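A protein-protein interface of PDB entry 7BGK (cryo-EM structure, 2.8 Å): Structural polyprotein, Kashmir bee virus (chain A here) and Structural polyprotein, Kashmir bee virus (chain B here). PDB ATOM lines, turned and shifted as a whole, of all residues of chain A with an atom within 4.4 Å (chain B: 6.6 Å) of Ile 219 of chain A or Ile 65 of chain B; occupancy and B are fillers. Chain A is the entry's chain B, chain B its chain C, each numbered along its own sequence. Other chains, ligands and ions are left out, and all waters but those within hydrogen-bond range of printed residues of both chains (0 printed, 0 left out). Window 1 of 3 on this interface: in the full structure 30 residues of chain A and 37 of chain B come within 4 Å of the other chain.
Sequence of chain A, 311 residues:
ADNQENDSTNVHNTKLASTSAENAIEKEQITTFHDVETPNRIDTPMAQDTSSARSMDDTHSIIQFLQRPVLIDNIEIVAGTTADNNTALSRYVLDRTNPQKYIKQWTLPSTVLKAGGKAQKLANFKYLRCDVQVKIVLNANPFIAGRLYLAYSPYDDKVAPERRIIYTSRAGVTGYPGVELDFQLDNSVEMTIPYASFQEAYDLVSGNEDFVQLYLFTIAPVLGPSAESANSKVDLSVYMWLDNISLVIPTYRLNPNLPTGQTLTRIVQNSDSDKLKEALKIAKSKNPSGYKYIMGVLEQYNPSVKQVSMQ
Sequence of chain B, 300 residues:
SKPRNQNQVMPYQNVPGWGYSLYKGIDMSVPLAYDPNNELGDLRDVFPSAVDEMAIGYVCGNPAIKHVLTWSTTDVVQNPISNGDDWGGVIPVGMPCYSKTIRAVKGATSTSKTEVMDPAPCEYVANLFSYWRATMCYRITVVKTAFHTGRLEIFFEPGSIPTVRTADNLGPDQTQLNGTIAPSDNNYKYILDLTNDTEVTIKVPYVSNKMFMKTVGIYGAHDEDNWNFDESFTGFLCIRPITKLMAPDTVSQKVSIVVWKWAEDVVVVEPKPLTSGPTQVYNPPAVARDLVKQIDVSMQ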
ATOM      1  N   ALA A  88      10.096  12.284  -9.641  1.00  0.00           N
ATOM      2  CA  ALA A  88      10.641  11.824 -10.900  1.00  0.00           C
ATOM      3  C   ALA A  88      11.989  12.472 -11.185  1.00  0.00           C
ATOM      4  O   ALA A  88      12.540  13.229 -10.383  1.00  0.00           O
ATOM      5  CB  ALA A  88       9.662  12.117 -12.025  1.00  0.00           C
ATOM      6  N   ARG A 147       7.817   3.817 -14.799  1.00  0.00           N
ATOM      7  CA  ARG A 147       9.048   3.539 -15.519  1.00  0.00           C
ATOM      8  C   ARG A 147      10.230   4.024 -14.700  1.00  0.00           C
ATOM      9  O   ARG A 147      10.267   5.186 -14.288  1.00  0.00           O
ATOM     10  CB  ARG A 147       9.049   4.214 -16.887  1.00  0.00           C
ATOM     11  CG  ARG A 147       9.835   3.473 -17.931  1.00  0.00           C
ATOM     12  CD  ARG A 147      10.058   4.311 -19.163  1.00  0.00           C
ATOM     13  NE  ARG A 147       9.069   4.076 -20.211  1.00  0.00           N
ATOM     14  CZ  ARG A 147       8.887   2.912 -20.823  1.00  0.00           C
ATOM     15  NH1 ARG A 147       9.625   1.863 -20.504  1.00  0.00           N
ATOM     16  NH2 ARG A 147       7.965   2.802 -21.761  1.00  0.00           N
ATOM     17  N   LEU A 148      11.186   3.134 -14.473  1.00  0.00           N
ATOM     18  CA  LEU A 148      12.423   3.442 -13.780  1.00  0.00           C
ATOM     19  C   LEU A 148      13.594   3.333 -14.746  1.00  0.00           C
ATOM     20  O   LEU A 148      13.473   2.803 -15.852  1.00  0.00           O
ATOM     21  CB  LEU A 148      12.625   2.504 -12.586  1.00  0.00           C
ATOM     22  CG  LEU A 148      11.406   2.248 -11.705  1.00  0.00           C
ATOM     23  CD1 LEU A 148      11.669   1.123 -10.749  1.00  0.00           C
ATOM     24  CD2 LEU A 148      11.041   3.486 -10.946  1.00  0.00           C
ATOM     25  N   TYR A 149      14.738   3.854 -14.318  1.00  0.00           N
ATOM     26  CA  TYR A 149      15.977   3.765 -15.081  1.00  0.00           C
ATOM     27  C   TYR A 149      17.092   3.366 -14.127  1.00  0.00           C
ATOM     28  O   TYR A 149      17.450   4.134 -13.230  1.00  0.00           O
ATOM     29  CB  TYR A 149      16.302   5.084 -15.775  1.00  0.00           C
ATOM     30  CG  TYR A 149      17.393   4.976 -16.814  1.00  0.00           C
ATOM     31  CD1 TYR A 149      17.182   4.287 -17.996  1.00  0.00           C
ATOM     32  CD2 TYR A 149      18.629   5.560 -16.618  1.00  0.00           C
ATOM     33  CE1 TYR A 149      18.168   4.184 -18.944  1.00  0.00           C
ATOM     34  CE2 TYR A 149      19.619   5.459 -17.562  1.00  0.00           C
ATOM     35  CZ  TYR A 149      19.383   4.769 -18.725  1.00  0.00           C
ATOM     36  OH  TYR A 149      20.362   4.663 -19.680  1.00  0.00           O
ATOM     37  N   ARG A 170      18.139  15.148 -16.989  1.00  0.00           N
ATOM     38  CA  ARG A 170      17.479  13.902 -17.347  1.00  0.00           C
ATOM     39  C   ARG A 170      18.077  13.311 -18.614  1.00  0.00           C
ATOM     40  O   ARG A 170      18.286  12.096 -18.705  1.00  0.00           O
ATOM     41  CB  ARG A 170      15.989  14.154 -17.522  1.00  0.00           C
ATOM     42  CG  ARG A 170      15.172  12.925 -17.736  1.00  0.00           C
ATOM     43  CD  ARG A 170      13.707  13.236 -17.652  1.00  0.00           C
ATOM     44  NE  ARG A 170      13.292  14.207 -18.654  1.00  0.00           N
ATOM     45  CZ  ARG A 170      12.167  14.906 -18.588  1.00  0.00           C
ATOM     46  NH1 ARG A 170      11.339  14.747 -17.571  1.00  0.00           N
ATOM     47  NH2 ARG A 170      11.872  15.765 -19.544  1.00  0.00           N
ATOM     48  N   ALA A 171      18.358  14.155 -19.605  1.00  0.00           N
ATOM     49  CA  ALA A 171      18.983  13.678 -20.826  1.00  0.00           C
ATOM     50  C   ALA A 171      20.429  13.275 -20.603  1.00  0.00           C
ATOM     51  O   ALA A 171      20.977  12.507 -21.398  1.00  0.00           O
ATOM     52  CB  ALA A 171      18.900  14.752 -21.906  1.00  0.00           C
ATOM     53  N   THR A 174      20.009   9.751 -18.482  1.00  0.00           N
ATOM     54  CA  THR A 174      19.643   8.696 -19.413  1.00  0.00           C
ATOM     55  C   THR A 174      20.656   8.504 -20.525  1.00  0.00           C
ATOM     56  O   THR A 174      20.479   7.604 -21.351  1.00  0.00           O
ATOM     57  CB  THR A 174      18.274   8.997 -19.999  1.00  0.00           C
ATOM     58  OG1 THR A 174      18.286  10.297 -20.593  1.00  0.00           O
ATOM     59  CG2 THR A 174      17.243   8.961 -18.911  1.00  0.00           C
ATOM     60  N   PHE A 217      16.796   5.398 -10.800  1.00  0.00           N
ATOM     61  CA  PHE A 217      16.083   6.646 -10.978  1.00  0.00           C
ATOM     62  C   PHE A 217      14.623   6.374 -11.318  1.00  0.00           C
ATOM     63  O   PHE A 217      14.191   5.232 -11.477  1.00  0.00           O
ATOM     64  CB  PHE A 217      16.751   7.484 -12.064  1.00  0.00           C
ATOM     65  CG  PHE A 217      18.114   7.973 -11.700  1.00  0.00           C
ATOM     66  CD1 PHE A 217      18.275   9.006 -10.803  1.00  0.00           C
ATOM     67  CD2 PHE A 217      19.236   7.409 -12.264  1.00  0.00           C
ATOM     68  CE1 PHE A 217      19.524   9.457 -10.475  1.00  0.00           C
ATOM     69  CE2 PHE A 217      20.482   7.861 -11.935  1.00  0.00           C
ATOM     70  CZ  PHE A 217      20.625   8.886 -11.039  1.00  0.00           C
ATOM     71  N   THR A 218      13.855   7.452 -11.429  1.00  0.00           N
ATOM     72  CA  THR A 218      12.430   7.387 -11.722  1.00  0.00           C
ATOM     73  C   THR A 218      12.134   8.292 -12.910  1.00  0.00           C
ATOM     74  O   THR A 218      12.236   9.516 -12.801  1.00  0.00           O
ATOM     75  CB  THR A 218      11.610   7.798 -10.502  1.00  0.00           C
ATOM     76  OG1 THR A 218      12.084   7.094  -9.349  1.00  0.00           O
ATOM     77  CG2 THR A 218      10.161   7.478 -10.695  1.00  0.00           C
ATOM     78  N   ILE A 219      11.785   7.690 -14.045  1.00  0.00           N
ATOM     79  CA  ILE A 219      11.376   8.466 -15.209  1.00  0.00           C
ATOM     80  C   ILE A 219       9.944   8.949 -15.045  1.00  0.00           C
ATOM     81  O   ILE A 219       9.659  10.146 -15.152  1.00  0.00           O
ATOM     82  CB  ILE A 219      11.542   7.631 -16.492  1.00  0.00           C
ATOM     83  CG1 ILE A 219      13.004   7.271 -16.727  1.00  0.00           C
ATOM     84  CG2 ILE A 219      11.010   8.380 -17.693  1.00  0.00           C
ATOM     85  CD1 ILE A 219      13.193   6.159 -17.717  1.00  0.00           C
ATOM     86  N   ALA A 220       9.029   8.022 -14.783  1.00  0.00           N
ATOM     87  CA  ALA A 220       7.636   8.318 -14.539  1.00  0.00           C
ATOM     88  C   ALA A 220       7.233   7.734 -13.193  1.00  0.00           C
ATOM     89  O   ALA A 220       7.442   6.536 -12.958  1.00  0.00           O
ATOM     90  CB  ALA A 220       6.750   7.738 -15.640  1.00  0.00           C
ATOM     91  N   PRO A 221       6.668   8.528 -12.287  1.00  0.00           N
ATOM     92  CA  PRO A 221       6.267   7.989 -10.986  1.00  0.00           C
ATOM     93  C   PRO A 221       5.157   6.959 -11.120  1.00  0.00           C
ATOM     94  O   PRO A 221       4.558   6.769 -12.179  1.00  0.00           O
ATOM     95  CB  PRO A 221       5.799   9.230 -10.225  1.00  0.00           C
ATOM     96  CG  PRO A 221       5.435  10.190 -11.258  1.00  0.00           C
ATOM     97  CD  PRO A 221       6.364   9.962 -12.388  1.00  0.00           C
ATOM     98  N   PRO B  63      20.930   6.989 -27.040  1.00  0.00           N
ATOM     99  CA  PRO B  63      19.715   7.780 -26.864  1.00  0.00           C
ATOM    100  C   PRO B  63      19.587   8.352 -25.462  1.00  0.00           C
ATOM    101  O   PRO B  63      20.194   7.879 -24.501  1.00  0.00           O
ATOM    102  CB  PRO B  63      18.598   6.777 -27.156  1.00  0.00           C
ATOM    103  CG  PRO B  63      19.175   5.472 -26.910  1.00  0.00           C
ATOM    104  CD  PRO B  63      20.633   5.553 -27.158  1.00  0.00           C
ATOM    105  N   ALA B  64      18.775   9.400 -25.370  1.00  0.00           N
ATOM    106  CA  ALA B  64      18.509  10.075 -24.114  1.00  0.00           C
ATOM    107  C   ALA B  64      17.082  10.595 -24.124  1.00  0.00           C
ATOM    108  O   ALA B  64      16.530  10.905 -25.181  1.00  0.00           O
ATOM    109  CB  ALA B  64      19.489  11.218 -23.882  1.00  0.00           C
ATOM    110  N   ILE B  65      16.495  10.687 -22.937  1.00  0.00           N
ATOM    111  CA  ILE B  65      15.118  11.144 -22.791  1.00  0.00           C
ATOM    112  C   ILE B  65      15.088  12.665 -22.841  1.00  0.00           C
ATOM    113  O   ILE B  65      15.691  13.337 -21.999  1.00  0.00           O
ATOM    114  CB  ILE B  65      14.489  10.611 -21.498  1.00  0.00           C
ATOM    115  CG1 ILE B  65      14.118   9.146 -21.675  1.00  0.00           C
ATOM    116  CG2 ILE B  65      13.262  11.405 -21.120  1.00  0.00           C
ATOM    117  CD1 ILE B  65      13.803   8.429 -20.416  1.00  0.00           C
ATOM    118  N   LYS B  66      14.376  13.206 -23.828  1.00  0.00           N
ATOM    119  CA  LYS B  66      14.222  14.639 -23.999  1.00  0.00           C
ATOM    120  C   LYS B  66      12.795  15.117 -23.784  1.00  0.00           C
ATOM    121  O   LYS B  66      12.582  16.324 -23.639  1.00  0.00           O
ATOM    122  CB  LYS B  66      14.683  15.050 -25.399  1.00  0.00           C
ATOM    123  CG  LYS B  66      16.178  15.008 -25.607  1.00  0.00           C
ATOM    124  CD  LYS B  66      16.887  16.169 -24.947  1.00  0.00           C
ATOM    125  CE  LYS B  66      16.507  17.477 -25.576  1.00  0.00           C
ATOM    126  NZ  LYS B  66      17.572  18.488 -25.457  1.00  0.00           N
ATOM    127  N   HIS B  67      11.823  14.211 -23.761  1.00  0.00           N
ATOM    128  CA  HIS B  67      10.425  14.543 -23.534  1.00  0.00           C
ATOM    129  C   HIS B  67       9.819  13.482 -22.635  1.00  0.00           C
ATOM    130  O   HIS B  67      10.008  12.287 -22.873  1.00  0.00           O
ATOM    131  CB  HIS B  67       9.623  14.605 -24.839  1.00  0.00           C
ATOM    132  CG  HIS B  67       9.948  15.773 -25.713  1.00  0.00           C
ATOM    133  ND1 HIS B  67       9.310  16.987 -25.590  1.00  0.00           N
ATOM    134  CD2 HIS B  67      10.812  15.905 -26.746  1.00  0.00           C
ATOM    135  CE1 HIS B  67       9.782  17.823 -26.496  1.00  0.00           C
ATOM    136  NE2 HIS B  67      10.692  17.191 -27.212  1.00  0.00           N
ATOM    137  N   VAL B  68       9.109  13.920 -21.602  1.00  0.00           N
ATOM    138  CA  VAL B  68       8.244  13.055 -20.811  1.00  0.00           C
ATOM    139  C   VAL B  68       6.941  13.817 -20.636  1.00  0.00           C
ATOM    140  O   VAL B  68       6.821  14.665 -19.746  1.00  0.00           O
ATOM    141  CB  VAL B  68       8.851  12.677 -19.458  1.00  0.00           C
ATOM    142  CG1 VAL B  68       7.989  11.657 -18.769  1.00  0.00           C
ATOM    143  CG2 VAL B  68      10.239  12.133 -19.631  1.00  0.00           C
ATOM    144  N   ASP B 118      19.893  21.286 -22.172  1.00  0.00           N
ATOM    145  CA  ASP B 118      19.630  19.890 -21.828  1.00  0.00           C
ATOM    146  C   ASP B 118      20.088  18.980 -22.964  1.00  0.00           C
ATOM    147  O   ASP B 118      19.259  18.373 -23.655  1.00  0.00           O
ATOM    148  CB  ASP B 118      18.139  19.698 -21.560  1.00  0.00           C
ATOM    149  CG  ASP B 118      17.839  18.450 -20.773  1.00  0.00           C
ATOM    150  OD1 ASP B 118      17.944  18.503 -19.538  1.00  0.00           O
ATOM    151  OD2 ASP B 118      17.481  17.422 -21.383  1.00  0.00           O
ATOM    152  N   ALA B 120      21.380  15.944 -25.259  1.00  0.00           N
ATOM    153  CA  ALA B 120      21.602  14.519 -25.415  1.00  0.00           C
ATOM    154  C   ALA B 120      22.953  14.296 -26.067  1.00  0.00           C
ATOM    155  O   ALA B 120      23.567  15.222 -26.598  1.00  0.00           O
ATOM    156  CB  ALA B 120      20.477  13.907 -26.242  1.00  0.00           C
ATOM    157  N   VAL B 143       3.986   5.016 -21.235  1.00  0.00           N
ATOM    158  CA  VAL B 143       3.937   4.302 -19.968  1.00  0.00           C
ATOM    159  C   VAL B 143       2.471   4.156 -19.589  1.00  0.00           C
ATOM    160  O   VAL B 143       1.813   5.134 -19.220  1.00  0.00           O
ATOM    161  CB  VAL B 143       4.725   5.032 -18.877  1.00  0.00           C
ATOM    162  CG1 VAL B 143       4.693   4.257 -17.613  1.00  0.00           C
ATOM    163  CG2 VAL B 143       6.144   5.259 -19.310  1.00  0.00           C
ATOM    164  N   SER B 256       2.221   8.554 -19.340  1.00  0.00           N
ATOM    165  CA  SER B 256       3.432   9.290 -19.657  1.00  0.00           C
ATOM    166  C   SER B 256       3.921   8.891 -21.041  1.00  0.00           C
ATOM    167  O   SER B 256       3.903   7.713 -21.401  1.00  0.00           O
ATOM    168  CB  SER B 256       4.517   9.029 -18.616  1.00  0.00           C
ATOM    169  OG  SER B 256       5.671   9.801 -18.879  1.00  0.00           O
ATOM    170  N   VAL B 258       7.185   9.038 -23.017  1.00  0.00           N
ATOM    171  CA  VAL B 258       8.629   9.214 -23.000  1.00  0.00           C
ATOM    172  C   VAL B 258       9.145   9.150 -24.427  1.00  0.00           C
ATOM    173  O   VAL B 258       8.693   8.326 -25.229  1.00  0.00           O
ATOM    174  CB  VAL B 258       9.295   8.145 -22.114  1.00  0.00           C
ATOM    175  CG1 VAL B 258      10.735   8.461 -21.898  1.00  0.00           C
ATOM    176  CG2 VAL B 258       8.579   8.027 -20.790  1.00  0.00           C
ATOM    177  N   VAL B 259      10.090  10.027 -24.753  1.00  0.00           N
ATOM    178  CA  VAL B 259      10.653  10.118 -26.092  1.00  0.00           C
ATOM    179  C   VAL B 259      12.169  10.115 -25.972  1.00  0.00           C
ATOM    180  O   VAL B 259      12.747  11.026 -25.371  1.00  0.00           O
ATOM    181  CB  VAL B 259      10.176  11.373 -26.842  1.00  0.00           C
ATOM    182  CG1 VAL B 259      10.629  11.346 -28.275  1.00  0.00           C
ATOM    183  CG2 VAL B 259       8.675  11.497 -26.776  1.00  0.00           C
ATOM    184  N   TRP B 260      12.805   9.094 -26.531  1.00  0.00           N
ATOM    185  CA  TRP B 260      14.252   9.043 -26.642  1.00  0.00           C
ATOM    186  C   TRP B 260      14.692   9.610 -27.983  1.00  0.00           C
ATOM    187  O   TRP B 260      14.003   9.474 -28.995  1.00  0.00           O
ATOM    188  CB  TRP B 260      14.759   7.611 -26.506  1.00  0.00           C
ATOM    189  CG  TRP B 260      14.392   6.932 -25.232  1.00  0.00           C
ATOM    190  CD1 TRP B 260      13.163   6.474 -24.876  1.00  0.00           C
ATOM    191  CD2 TRP B 260      15.266   6.612 -24.148  1.00  0.00           C
ATOM    192  NE1 TRP B 260      13.213   5.897 -23.639  1.00  0.00           N
ATOM    193  CE2 TRP B 260      14.496   5.968 -23.169  1.00  0.00           C
ATOM    194  CE3 TRP B 260      16.626   6.811 -23.909  1.00  0.00           C
ATOM    195  CZ2 TRP B 260      15.039   5.524 -21.972  1.00  0.00           C
ATOM    196  CZ3 TRP B 260      17.158   6.371 -22.727  1.00  0.00           C
ATOM    197  CH2 TRP B 260      16.370   5.736 -21.773  1.00  0.00           C
ATOM    198  N   LYS B 261      15.859  10.243 -27.983  1.00  0.00           N
ATOM    199  CA  LYS B 261      16.383  10.925 -29.152  1.00  0.00           C
ATOM    200  C   LYS B 261      17.796  10.453 -29.453  1.00  0.00           C
ATOM    201  O   LYS B 261      18.626  10.335 -28.549  1.00  0.00           O
ATOM    202  CB  LYS B 261      16.375  12.434 -28.941  1.00  0.00           C
ATOM    203  CG  LYS B 261      17.007  13.227 -30.049  1.00  0.00           C
ATOM    204  CD  LYS B 261      16.946  14.699 -29.768  1.00  0.00           C
ATOM    205  CE  LYS B 261      17.733  15.478 -30.779  1.00  0.00           C
ATOM    206  NZ  LYS B 261      17.384  16.908 -30.758  1.00  0.00           N
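N of Ile 65 of chain B is in hydrogen-bond range of OG1 of Thr 174 of chain A, at 3.0 Å. The backbone carbonyl oxygen of Thr 174 of chain A lies close to the backbone carbonyl oxygen of Pro 63 of chain B.
Of the printed residues of chain B, Ala 171 of chain A touches Ala 64 (3.2 Å), Ile 65 (3.5 Å), Lys 66 (3.9 Å) and Asp 118 (3.1 Å). Of the printed residues of chain A, Ala 64 of chain B touches Ala 171 and Thr 174. Of chain A, only Arg 170, Ala 171, Thr 174 and Ile 219 come within 4 Å of Ile 65 of chain B. Of the printed residues of chain A, Val 258 of chain B touches Ile 219. The nearest residue of chain B that does not touch Ile 219 of chain A is Val 68 of chain B (4.3 Å). The nearest printed residue of chain A that does not touch Ile 65 of chain B is Arg 147 of chain A (5.7 Å). The nearest printed residue of chain A that does not touch Ser 256 of chain B is Ile 219 of chain A (5.5 Å).
Printed residues of chain B that touch a printed residue of chain A: Pro 63, Ala 64, Ile 65, Lys 66, Val 68, Asp 118, Val 143, Ser 256, Val 258 and Trp 260. Along chain B the printed residues that touch a printed residue of chain A span positions 63 to 260. Of the 12 printed residues of chain A, 7 touch a printed residue of chain B. Hydrophobic or aromatic side chains of chain A within 4 Å of the printed part of chain B: Tyr 149, Ala 171, Ile 219 and Ala 220. Among the printed residues, 15 pairs touch across the chains. Among the printed residues, no Asp or Glu carboxylate lies within 4 Å of a Lys or Arg side-chain nitrogen of the other chain.
The side-chain amino group of Lys 66 of chain B lies within hydrogen-bond range of the backbone carbonyl oxygen of Asp 118 of chain B (2.5 Å). The backbone NH of Lys 66 of chain B is in hydrogen-bond range of the backbone carbonyl oxygen of Val 259 of chain B, 3.1 Å away. O of Ser 256 of chain B lies within hydrogen-bond range of N of Val 143 of chain B, at 2.7 Å. N of Ile 219 of chain A is in hydrogen-bond range of O of Arg 147 of chain A (2.9 Å). The backbone NH of Ala 220 of chain A sits at hydrogen-bond distance from the backbone carbonyl oxygen of Arg 147 of chain A (3.1 Å). The side-chain hydroxyl (OG1) of Thr 174 of chain A sits at hydrogen-bond distance from the backbone carbonyl oxygen (O) of Arg 170 of chain A (2.6 Å).
Trp 260 of chain B touches Tyr 149 of chain A (CH2 to CE1, 3.7 Å). Ile 65 of chain B touches Arg 170 of chain A (CG2 to NE, 3.7 Å). NH1 of Arg 170 of chain A touches CG2 of Val 68 of chain B, 3.5 Å away. CB of Ala 171 of chain A touches O of Ile 65 of chain B (3.5 Å). CB of Ala 171 of chain A touches CD of Lys 66 of chain B (3.9 Å). CB of Ala 171 of chain A touches OD2 of Asp 118 of chain B (3.1 Å). CA of Ala 64 of chain B touches OG1 of Thr 174 of chain A, at 3.5 Å. O of Thr 174 of chain A touches CZ3 of Trp 260 of chain B, at 3.8 Å. CG2 of Ile 219 of chain A touches CG2 of Val 258 of chain B, 3.95 Å away. CB of Ser 256 of chain B touches CB of Ala 220 of chain A (3.9 Å).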
